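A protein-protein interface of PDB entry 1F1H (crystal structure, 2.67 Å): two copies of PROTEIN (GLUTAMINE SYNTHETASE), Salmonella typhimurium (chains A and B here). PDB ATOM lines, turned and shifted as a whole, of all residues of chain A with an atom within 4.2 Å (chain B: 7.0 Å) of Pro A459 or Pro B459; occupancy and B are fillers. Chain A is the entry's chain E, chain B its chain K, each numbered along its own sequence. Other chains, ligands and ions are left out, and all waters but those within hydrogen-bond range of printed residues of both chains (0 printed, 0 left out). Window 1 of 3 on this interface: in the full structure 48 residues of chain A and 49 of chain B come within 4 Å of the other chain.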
ATOM      1  N   SER A 147      10.907 -20.174  17.275  1.00  0.00           N
ATOM      2  CA  SER A 147      11.095 -20.024  18.716  1.00  0.00           C
ATOM      3  C   SER A 147      12.035 -18.866  18.925  1.00  0.00           C
ATOM      4  O   SER A 147      12.748 -18.470  18.004  1.00  0.00           O
ATOM      5  CB  SER A 147      11.749 -21.280  19.347  1.00  0.00           C
ATOM      6  OG  SER A 147      12.328 -22.179  18.391  1.00  0.00           O
ATOM      7  N   HIS A 148      12.054 -18.335  20.141  1.00  0.00           N
ATOM      8  CA  HIS A 148      12.966 -17.253  20.453  1.00  0.00           C
ATOM      9  C   HIS A 148      12.963 -16.911  21.924  1.00  0.00           C
ATOM     10  O   HIS A 148      12.020 -17.224  22.649  1.00  0.00           O
ATOM     11  CB  HIS A 148      12.600 -15.991  19.673  1.00  0.00           C
ATOM     12  CG  HIS A 148      11.423 -15.258  20.237  1.00  0.00           C
ATOM     13  ND1 HIS A 148      10.122 -15.647  20.000  1.00  0.00           N
ATOM     14  CD2 HIS A 148      11.352 -14.180  21.060  1.00  0.00           C
ATOM     15  CE1 HIS A 148       9.300 -14.844  20.655  1.00  0.00           C
ATOM     16  NE2 HIS A 148      10.020 -13.946  21.304  1.00  0.00           N
ATOM     17  N   PRO A 457      12.667 -27.911  17.681  1.00  0.00           N
ATOM     18  CA  PRO A 457      13.892 -27.457  17.013  1.00  0.00           C
ATOM     19  C   PRO A 457      14.498 -26.248  17.728  1.00  0.00           C
ATOM     20  O   PRO A 457      13.785 -25.318  18.114  1.00  0.00           O
ATOM     21  CB  PRO A 457      13.404 -27.091  15.613  1.00  0.00           C
ATOM     22  CG  PRO A 457      12.273 -28.017  15.396  1.00  0.00           C
ATOM     23  CD  PRO A 457      11.552 -27.978  16.724  1.00  0.00           C
ATOM     24  N   HIS A 458      15.816 -26.294  17.889  1.00  0.00           N
ATOM     25  CA  HIS A 458      16.611 -25.266  18.561  1.00  0.00           C
ATOM     26  C   HIS A 458      17.243 -24.330  17.545  1.00  0.00           C
ATOM     27  O   HIS A 458      17.849 -24.780  16.584  1.00  0.00           O
ATOM     28  CB  HIS A 458      17.729 -25.955  19.360  1.00  0.00           C
ATOM     29  CG  HIS A 458      18.571 -25.032  20.190  1.00  0.00           C
ATOM     30  ND1 HIS A 458      18.797 -25.246  21.533  1.00  0.00           N
ATOM     31  CD2 HIS A 458      19.260 -23.913  19.867  1.00  0.00           C
ATOM     32  CE1 HIS A 458      19.585 -24.296  22.003  1.00  0.00           C
ATOM     33  NE2 HIS A 458      19.881 -23.473  21.011  1.00  0.00           N
ATOM     34  N   PRO A 459      17.174 -23.014  17.795  1.00  0.00           N
ATOM     35  CA  PRO A 459      17.727 -21.954  16.947  1.00  0.00           C
ATOM     36  C   PRO A 459      19.110 -22.266  16.395  1.00  0.00           C
ATOM     37  O   PRO A 459      19.359 -22.089  15.203  1.00  0.00           O
ATOM     38  CB  PRO A 459      17.778 -20.775  17.903  1.00  0.00           C
ATOM     39  CG  PRO A 459      16.510 -20.955  18.667  1.00  0.00           C
ATOM     40  CD  PRO A 459      16.490 -22.433  18.965  1.00  0.00           C
ATOM     41  N   VAL A 460      19.981 -22.778  17.268  1.00  0.00           N
ATOM     42  CA  VAL A 460      21.361 -23.134  16.928  1.00  0.00           C
ATOM     43  C   VAL A 460      21.457 -24.253  15.874  1.00  0.00           C
ATOM     44  O   VAL A 460      22.439 -24.351  15.121  1.00  0.00           O
ATOM     45  CB  VAL A 460      22.152 -23.487  18.227  1.00  0.00           C
ATOM     46  CG1 VAL A 460      23.492 -24.107  17.918  1.00  0.00           C
ATOM     47  CG2 VAL A 460      22.386 -22.218  19.041  1.00  0.00           C
ATOM     48  N   GLU A 461      20.410 -25.068  15.795  1.00  0.00           N
ATOM     49  CA  GLU A 461      20.362 -26.161  14.824  1.00  0.00           C
ATOM     50  C   GLU A 461      20.245 -25.615  13.410  1.00  0.00           C
ATOM     51  O   GLU A 461      20.619 -26.267  12.441  1.00  0.00           O
ATOM     52  CB  GLU A 461      19.201 -27.110  15.137  1.00  0.00           C
ATOM     53  CG  GLU A 461      19.410 -27.903  16.437  1.00  0.00           C
ATOM     54  CD  GLU A 461      18.315 -28.930  16.736  1.00  0.00           C
ATOM     55  OE1 GLU A 461      18.639 -29.976  17.330  1.00  0.00           O
ATOM     56  OE2 GLU A 461      17.131 -28.693  16.417  1.00  0.00           O
ATOM     57  N   PHE A 462      19.716 -24.401  13.303  1.00  0.00           N
ATOM     58  CA  PHE A 462      19.603 -23.757  12.013  1.00  0.00           C
ATOM     59  C   PHE A 462      20.939 -23.183  11.597  1.00  0.00           C
ATOM     60  O   PHE A 462      21.322 -23.244  10.424  1.00  0.00           O
ATOM     61  CB  PHE A 462      18.519 -22.662  12.059  1.00  0.00           C
ATOM     62  CG  PHE A 462      17.159 -23.292  12.206  1.00  0.00           C
ATOM     63  CD1 PHE A 462      16.383 -23.511  11.064  1.00  0.00           C
ATOM     64  CD2 PHE A 462      16.661 -23.690  13.439  1.00  0.00           C
ATOM     65  CE1 PHE A 462      15.145 -24.135  11.162  1.00  0.00           C
ATOM     66  CE2 PHE A 462      15.411 -24.315  13.535  1.00  0.00           C
ATOM     67  CZ  PHE A 462      14.662 -24.541  12.408  1.00  0.00           C
ATOM     68  N   GLU A 463      21.653 -22.635  12.576  1.00  0.00           N
ATOM     69  CA  GLU A 463      22.967 -22.031  12.375  1.00  0.00           C
ATOM     70  C   GLU A 463      23.885 -23.118  11.844  1.00  0.00           C
ATOM     71  O   GLU A 463      24.613 -22.928  10.864  1.00  0.00           O
ATOM     72  CB  GLU A 463      23.491 -21.533  13.727  1.00  0.00           C
ATOM     73  CG  GLU A 463      24.687 -20.598  13.697  1.00  0.00           C
ATOM     74  CD  GLU A 463      24.658 -19.658  14.867  1.00  0.00           C
ATOM     75  OE1 GLU A 463      24.191 -18.502  14.719  1.00  0.00           O
ATOM     76  OE2 GLU A 463      25.088 -20.094  15.948  1.00  0.00           O
ATOM     77  N   ARG B 139      15.214 -16.868   9.163  1.00  0.00           N
ATOM     78  CA  ARG B 139      16.064 -16.022   9.985  1.00  0.00           C
ATOM     79  C   ARG B 139      16.368 -16.739  11.290  1.00  0.00           C
ATOM     80  O   ARG B 139      15.537 -17.474  11.827  1.00  0.00           O
ATOM     81  CB  ARG B 139      15.392 -14.672  10.241  1.00  0.00           C
ATOM     82  CG  ARG B 139      15.457 -13.683   9.058  1.00  0.00           C
ATOM     83  CD  ARG B 139      14.223 -12.772   8.955  1.00  0.00           C
ATOM     84  NE  ARG B 139      13.636 -12.463  10.257  1.00  0.00           N
ATOM     85  CZ  ARG B 139      12.373 -12.724  10.574  1.00  0.00           C
ATOM     86  NH1 ARG B 139      11.913 -12.433  11.785  1.00  0.00           N
ATOM     87  NH2 ARG B 139      11.566 -13.274   9.673  1.00  0.00           N
ATOM     88  N   PHE B 140      17.595 -16.575  11.758  1.00  0.00           N
ATOM     89  CA  PHE B 140      18.016 -17.204  12.995  1.00  0.00           C
ATOM     90  C   PHE B 140      19.294 -16.577  13.541  1.00  0.00           C
ATOM     91  O   PHE B 140      20.008 -15.860  12.838  1.00  0.00           O
ATOM     92  CB  PHE B 140      18.188 -18.710  12.794  1.00  0.00           C
ATOM     93  CG  PHE B 140      19.214 -19.078  11.760  1.00  0.00           C
ATOM     94  CD1 PHE B 140      20.582 -18.977  12.045  1.00  0.00           C
ATOM     95  CD2 PHE B 140      18.818 -19.494  10.485  1.00  0.00           C
ATOM     96  CE1 PHE B 140      21.543 -19.278  11.073  1.00  0.00           C
ATOM     97  CE2 PHE B 140      19.766 -19.798   9.506  1.00  0.00           C
ATOM     98  CZ  PHE B 140      21.137 -19.685   9.805  1.00  0.00           C
ATOM     99  N   GLY B 141      19.575 -16.849  14.806  1.00  0.00           N
ATOM    100  CA  GLY B 141      20.761 -16.295  15.423  1.00  0.00           C
ATOM    101  C   GLY B 141      20.861 -16.681  16.877  1.00  0.00           C
ATOM    102  O   GLY B 141      19.881 -17.133  17.477  1.00  0.00           O
ATOM    103  N   ALA B 142      22.055 -16.508  17.437  1.00  0.00           N
ATOM    104  CA  ALA B 142      22.314 -16.818  18.839  1.00  0.00           C
ATOM    105  C   ALA B 142      23.462 -15.953  19.304  1.00  0.00           C
ATOM    106  O   ALA B 142      24.502 -15.869  18.640  1.00  0.00           O
ATOM    107  CB  ALA B 142      22.662 -18.275  19.010  1.00  0.00           C
ATOM    108  N   GLY B 146      20.423 -13.995  23.831  1.00  0.00           N
ATOM    109  CA  GLY B 146      19.312 -14.805  23.343  1.00  0.00           C
ATOM    110  C   GLY B 146      19.571 -15.613  22.080  1.00  0.00           C
ATOM    111  O   GLY B 146      20.703 -15.716  21.593  1.00  0.00           O
ATOM    112  N   SER B 147      18.496 -16.182  21.545  1.00  0.00           N
ATOM    113  CA  SER B 147      18.540 -17.002  20.337  1.00  0.00           C
ATOM    114  C   SER B 147      17.182 -16.917  19.693  1.00  0.00           C
ATOM    115  O   SER B 147      16.206 -16.543  20.343  1.00  0.00           O
ATOM    116  CB  SER B 147      18.814 -18.493  20.662  1.00  0.00           C
ATOM    117  OG  SER B 147      18.648 -18.828  22.046  1.00  0.00           O
ATOM    118  N   HIS B 148      17.111 -17.283  18.418  1.00  0.00           N
ATOM    119  CA  HIS B 148      15.837 -17.288  17.728  1.00  0.00           C
ATOM    120  C   HIS B 148      15.936 -17.903  16.353  1.00  0.00           C
ATOM    121  O   HIS B 148      17.016 -17.987  15.770  1.00  0.00           O
ATOM    122  CB  HIS B 148      15.296 -15.867  17.574  1.00  0.00           C
ATOM    123  CG  HIS B 148      15.962 -15.086  16.487  1.00  0.00           C
ATOM    124  ND1 HIS B 148      17.190 -14.481  16.652  1.00  0.00           N
ATOM    125  CD2 HIS B 148      15.591 -14.843  15.204  1.00  0.00           C
ATOM    126  CE1 HIS B 148      17.549 -13.903  15.518  1.00  0.00           C
ATOM    127  NE2 HIS B 148      16.597 -14.106  14.624  1.00  0.00           N
ATOM    128  N   VAL B 149      14.788 -18.366  15.874  1.00  0.00           N
ATOM    129  CA  VAL B 149      14.631 -18.904  14.533  1.00  0.00           C
ATOM    130  C   VAL B 149      13.215 -18.555  14.104  1.00  0.00           C
ATOM    131  O   VAL B 149      12.262 -18.728  14.870  1.00  0.00           O
ATOM    132  CB  VAL B 149      14.839 -20.423  14.418  1.00  0.00           C
ATOM    133  CG1 VAL B 149      13.947 -21.181  15.358  1.00  0.00           C
ATOM    134  CG2 VAL B 149      14.518 -20.850  13.001  1.00  0.00           C
ATOM    135  N   MET B 256      17.376 -29.900   6.216  1.00  0.00           N
ATOM    136  CA  MET B 256      17.345 -30.166   7.656  1.00  0.00           C
ATOM    137  C   MET B 256      16.280 -31.217   7.901  1.00  0.00           C
ATOM    138  O   MET B 256      15.170 -31.143   7.352  1.00  0.00           O
ATOM    139  CB  MET B 256      16.848 -28.967   8.446  1.00  0.00           C
ATOM    140  CG  MET B 256      17.764 -27.834   8.640  1.00  0.00           C
ATOM    141  SD  MET B 256      16.779 -26.679   9.571  1.00  0.00           S
ATOM    142  CE  MET B 256      17.136 -27.244  11.225  1.00  0.00           C
ATOM    143  N   THR B 456      23.977 -24.258  24.722  1.00  0.00           N
ATOM    144  CA  THR B 456      23.201 -23.027  24.499  1.00  0.00           C
ATOM    145  C   THR B 456      21.755 -23.080  25.008  1.00  0.00           C
ATOM    146  O   THR B 456      20.964 -23.888  24.535  1.00  0.00           O
ATOM    147  CB  THR B 456      23.153 -22.691  22.987  1.00  0.00           C
ATOM    148  OG1 THR B 456      24.485 -22.551  22.469  1.00  0.00           O
ATOM    149  CG2 THR B 456      22.374 -21.420  22.744  1.00  0.00           C
ATOM    150  N   PRO B 457      21.366 -22.164  25.915  1.00  0.00           N
ATOM    151  CA  PRO B 457      19.989 -22.179  26.427  1.00  0.00           C
ATOM    152  C   PRO B 457      18.973 -22.164  25.283  1.00  0.00           C
ATOM    153  O   PRO B 457      19.121 -21.414  24.313  1.00  0.00           O
ATOM    154  CB  PRO B 457      19.917 -20.896  27.253  1.00  0.00           C
ATOM    155  CG  PRO B 457      21.303 -20.729  27.738  1.00  0.00           C
ATOM    156  CD  PRO B 457      22.126 -21.056  26.514  1.00  0.00           C
ATOM    157  N   HIS B 458      17.954 -23.005  25.427  1.00  0.00           N
ATOM    158  CA  HIS B 458      16.874 -23.181  24.456  1.00  0.00           C
ATOM    159  C   HIS B 458      15.653 -22.377  24.863  1.00  0.00           C
ATOM    160  O   HIS B 458      15.218 -22.447  26.003  1.00  0.00           O
ATOM    161  CB  HIS B 458      16.493 -24.670  24.413  1.00  0.00           C
ATOM    162  CG  HIS B 458      15.463 -25.027  23.383  1.00  0.00           C
ATOM    163  ND1 HIS B 458      15.655 -26.039  22.466  1.00  0.00           N
ATOM    164  CD2 HIS B 458      14.228 -24.529  23.140  1.00  0.00           C
ATOM    165  CE1 HIS B 458      14.585 -26.147  21.700  1.00  0.00           C
ATOM    166  NE2 HIS B 458      13.702 -25.242  22.089  1.00  0.00           N
ATOM    167  N   PRO B 459      15.038 -21.665  23.907  1.00  0.00           N
ATOM    168  CA  PRO B 459      13.845 -20.834  24.094  1.00  0.00           C
ATOM    169  C   PRO B 459      12.781 -21.475  24.972  1.00  0.00           C
ATOM    170  O   PRO B 459      12.252 -20.831  25.879  1.00  0.00           O
ATOM    171  CB  PRO B 459      13.344 -20.671  22.670  1.00  0.00           C
ATOM    172  CG  PRO B 459      14.623 -20.517  21.919  1.00  0.00           C
ATOM    173  CD  PRO B 459      15.505 -21.589  22.509  1.00  0.00           C
ATOM    174  N   VAL B 460      12.520 -22.760  24.725  1.00  0.00           N
ATOM    175  CA  VAL B 460      11.522 -23.546  25.457  1.00  0.00           C
ATOM    176  C   VAL B 460      11.853 -23.698  26.954  1.00  0.00           C
ATOM    177  O   VAL B 460      10.960 -23.874  27.799  1.00  0.00           O
ATOM    178  CB  VAL B 460      11.322 -24.928  24.760  1.00  0.00           C
ATOM    179  CG1 VAL B 460      10.508 -25.872  25.611  1.00  0.00           C
ATOM    180  CG2 VAL B 460      10.595 -24.729  23.434  1.00  0.00           C
ATOM    181  N   GLU B 461      13.135 -23.585  27.281  1.00  0.00           N
ATOM    182  CA  GLU B 461      13.584 -23.688  28.669  1.00  0.00           C
ATOM    183  C   GLU B 461      13.109 -22.490  29.476  1.00  0.00           C
ATOM    184  O   GLU B 461      12.973 -22.554  30.693  1.00  0.00           O
ATOM    185  CB  GLU B 461      15.110 -23.816  28.736  1.00  0.00           C
ATOM    186  CG  GLU B 461      15.623 -25.152  28.177  1.00  0.00           C
ATOM    187  CD  GLU B 461      17.135 -25.357  28.311  1.00  0.00           C
ATOM    188  OE1 GLU B 461      17.557 -26.517  28.484  1.00  0.00           O
ATOM    189  OE2 GLU B 461      17.908 -24.382  28.211  1.00  0.00           O
ATOM    190  N   PHE B 462      12.856 -21.390  28.778  1.00  0.00           N
ATOM    191  CA  PHE B 462      12.347 -20.202  29.429  1.00  0.00           C
ATOM    192  C   PHE B 462      10.866 -20.346  29.691  1.00  0.00           C
ATOM    193  O   PHE B 462      10.359 -19.933  30.741  1.00  0.00           O
ATOM    194  CB  PHE B 462      12.643 -18.957  28.572  1.00  0.00           C
ATOM    195  CG  PHE B 462      14.124 -18.684  28.554  1.00  0.00           C
ATOM    196  CD1 PHE B 462      14.656 -17.753  29.449  1.00  0.00           C
ATOM    197  CD2 PHE B 462      14.985 -19.353  27.693  1.00  0.00           C
ATOM    198  CE1 PHE B 462      16.025 -17.515  29.490  1.00  0.00           C
ATOM    199  CE2 PHE B 462      16.364 -19.107  27.735  1.00  0.00           C
ATOM    200  CZ  PHE B 462      16.880 -18.204  28.627  1.00  0.00           C
ATOM    201  N   GLU B 463      10.172 -20.948  28.728  1.00  0.00           N
ATOM    202  CA  GLU B 463       8.734 -21.181  28.796  1.00  0.00           C
ATOM    203  C   GLU B 463       8.476 -22.058  30.009  1.00  0.00           C
ATOM    204  O   GLU B 463       7.590 -21.787  30.826  1.00  0.00           O
ATOM    205  CB  GLU B 463       8.294 -21.920  27.527  1.00  0.00           C
ATOM    206  CG  GLU B 463       6.803 -21.980  27.248  1.00  0.00           C
ATOM    207  CD  GLU B 463       6.539 -22.040  25.771  1.00  0.00           C
ATOM    208  OE1 GLU B 463       6.260 -20.986  25.150  1.00  0.00           O
ATOM    209  OE2 GLU B 463       6.636 -23.153  25.228  1.00  0.00           O
ATOM    210  N   LEU B 464       9.328 -23.070  30.125  1.00  0.00           N
ATOM    211  CA  LEU B 464       9.307 -24.102  31.182  1.00  0.00           C
ATOM    212  C   LEU B 464       9.915 -23.684  32.516  1.00  0.00           C
ATOM    213  O   LEU B 464       9.400 -24.058  33.562  1.00  0.00           O
ATOM    214  CB  LEU B 464      10.121 -25.319  30.713  1.00  0.00           C
ATOM    215  CG  LEU B 464       9.457 -26.596  30.169  1.00  0.00           C
ATOM    216  CD1 LEU B 464       8.078 -26.302  29.617  1.00  0.00           C
ATOM    217  CD2 LEU B 464      10.336 -27.242  29.109  1.00  0.00           C
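O of Ser A147 lies within hydrogen-bond range of N of Val B149.
A ring nitrogen (ND1) of His A458 lies within hydrogen-bond range of a ring nitrogen (ND1) of His B458 (3.4 Å).
The backbone carbonyl oxygen (O) of Pro A457 sits at hydrogen-bond distance from the side-chain hydroxyl (OG) of Ser A147, at 3.5 Å.
N of His A458 lies within hydrogen-bond range of OE2 of Glu A461.
The backbone carbonyl oxygen (O) of Gly B141 lies within hydrogen-bond range of the backbone NH (N) of His B148, 2.9 Å away.
The backbone carbonyl oxygen (O) of Pro B457 is in hydrogen-bond range of the side-chain hydroxyl (OG) of Ser B147.
The backbone NH (N) of His B458 sits at hydrogen-bond distance from the side-chain carboxylate (OE2) of Glu B461 (3.1 Å).
CB of Pro B459 touches CB of Ser A147, at 3.7 Å.
His A148 touches Ser B147.
His B458 touches Pro A457.
His A458 touches Pro B457 (CE1 to O, 3.7 Å).
Pro A459 touches Ser B147.
O of His B148 touches CB of Pro A459 (3.6 Å).
Pro A459 touches Pro B459 (CD to CD, 3.8 Å).
Ala B142 touches Val A460.
Glu A461 touches Met B256.
Phe A462 touches Val B149 (CD2 to CG2, 3.6 Å).
Of the printed residues of chain B, Ser A147 touches His B148, Val B149 and Pro B459.
Pro A459 touches just these residues of chain B: Ser B147, His B148 and Pro B459.
Of the printed residues of chain A, Ala B142 touches Val A460 and Glu A463.
Of the printed residues of chain A, Pro B459 touches Ser A147, His A148 and Pro A459.
Leu B464 touches none of the printed residues of chain A.
Of the 18 printed residues of chain B, 10 touch a printed residue of chain A.
Printed residues of chain A that touch a printed residue of chain B: Ser A147, His A148, Pro A457, His A458, Pro A459, Val A460, Glu A461, Phe A462 and Glu A463.
Among the printed residues, 21 pairs touch across the chains.
Among the printed residues, no Asp or Glu carboxylate lies within 4 Å of a Lys or Arg side-chain nitrogen of the other chain.
Ser A147 touches His B148, and with the chains exchanged His A148 touches Ser B147.
Ser A147 touches Pro B459, and with the chains exchanged Pro A459 touches Ser B147.
His B148 touches its own counterpart, His A148.
His A148 touches Pro B459, and with the chains exchanged Pro A459 touches His B148.
Of the 21 pairs that touch across the chains among the printed residues, 11 have their exchanged pair printed and touching as well.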
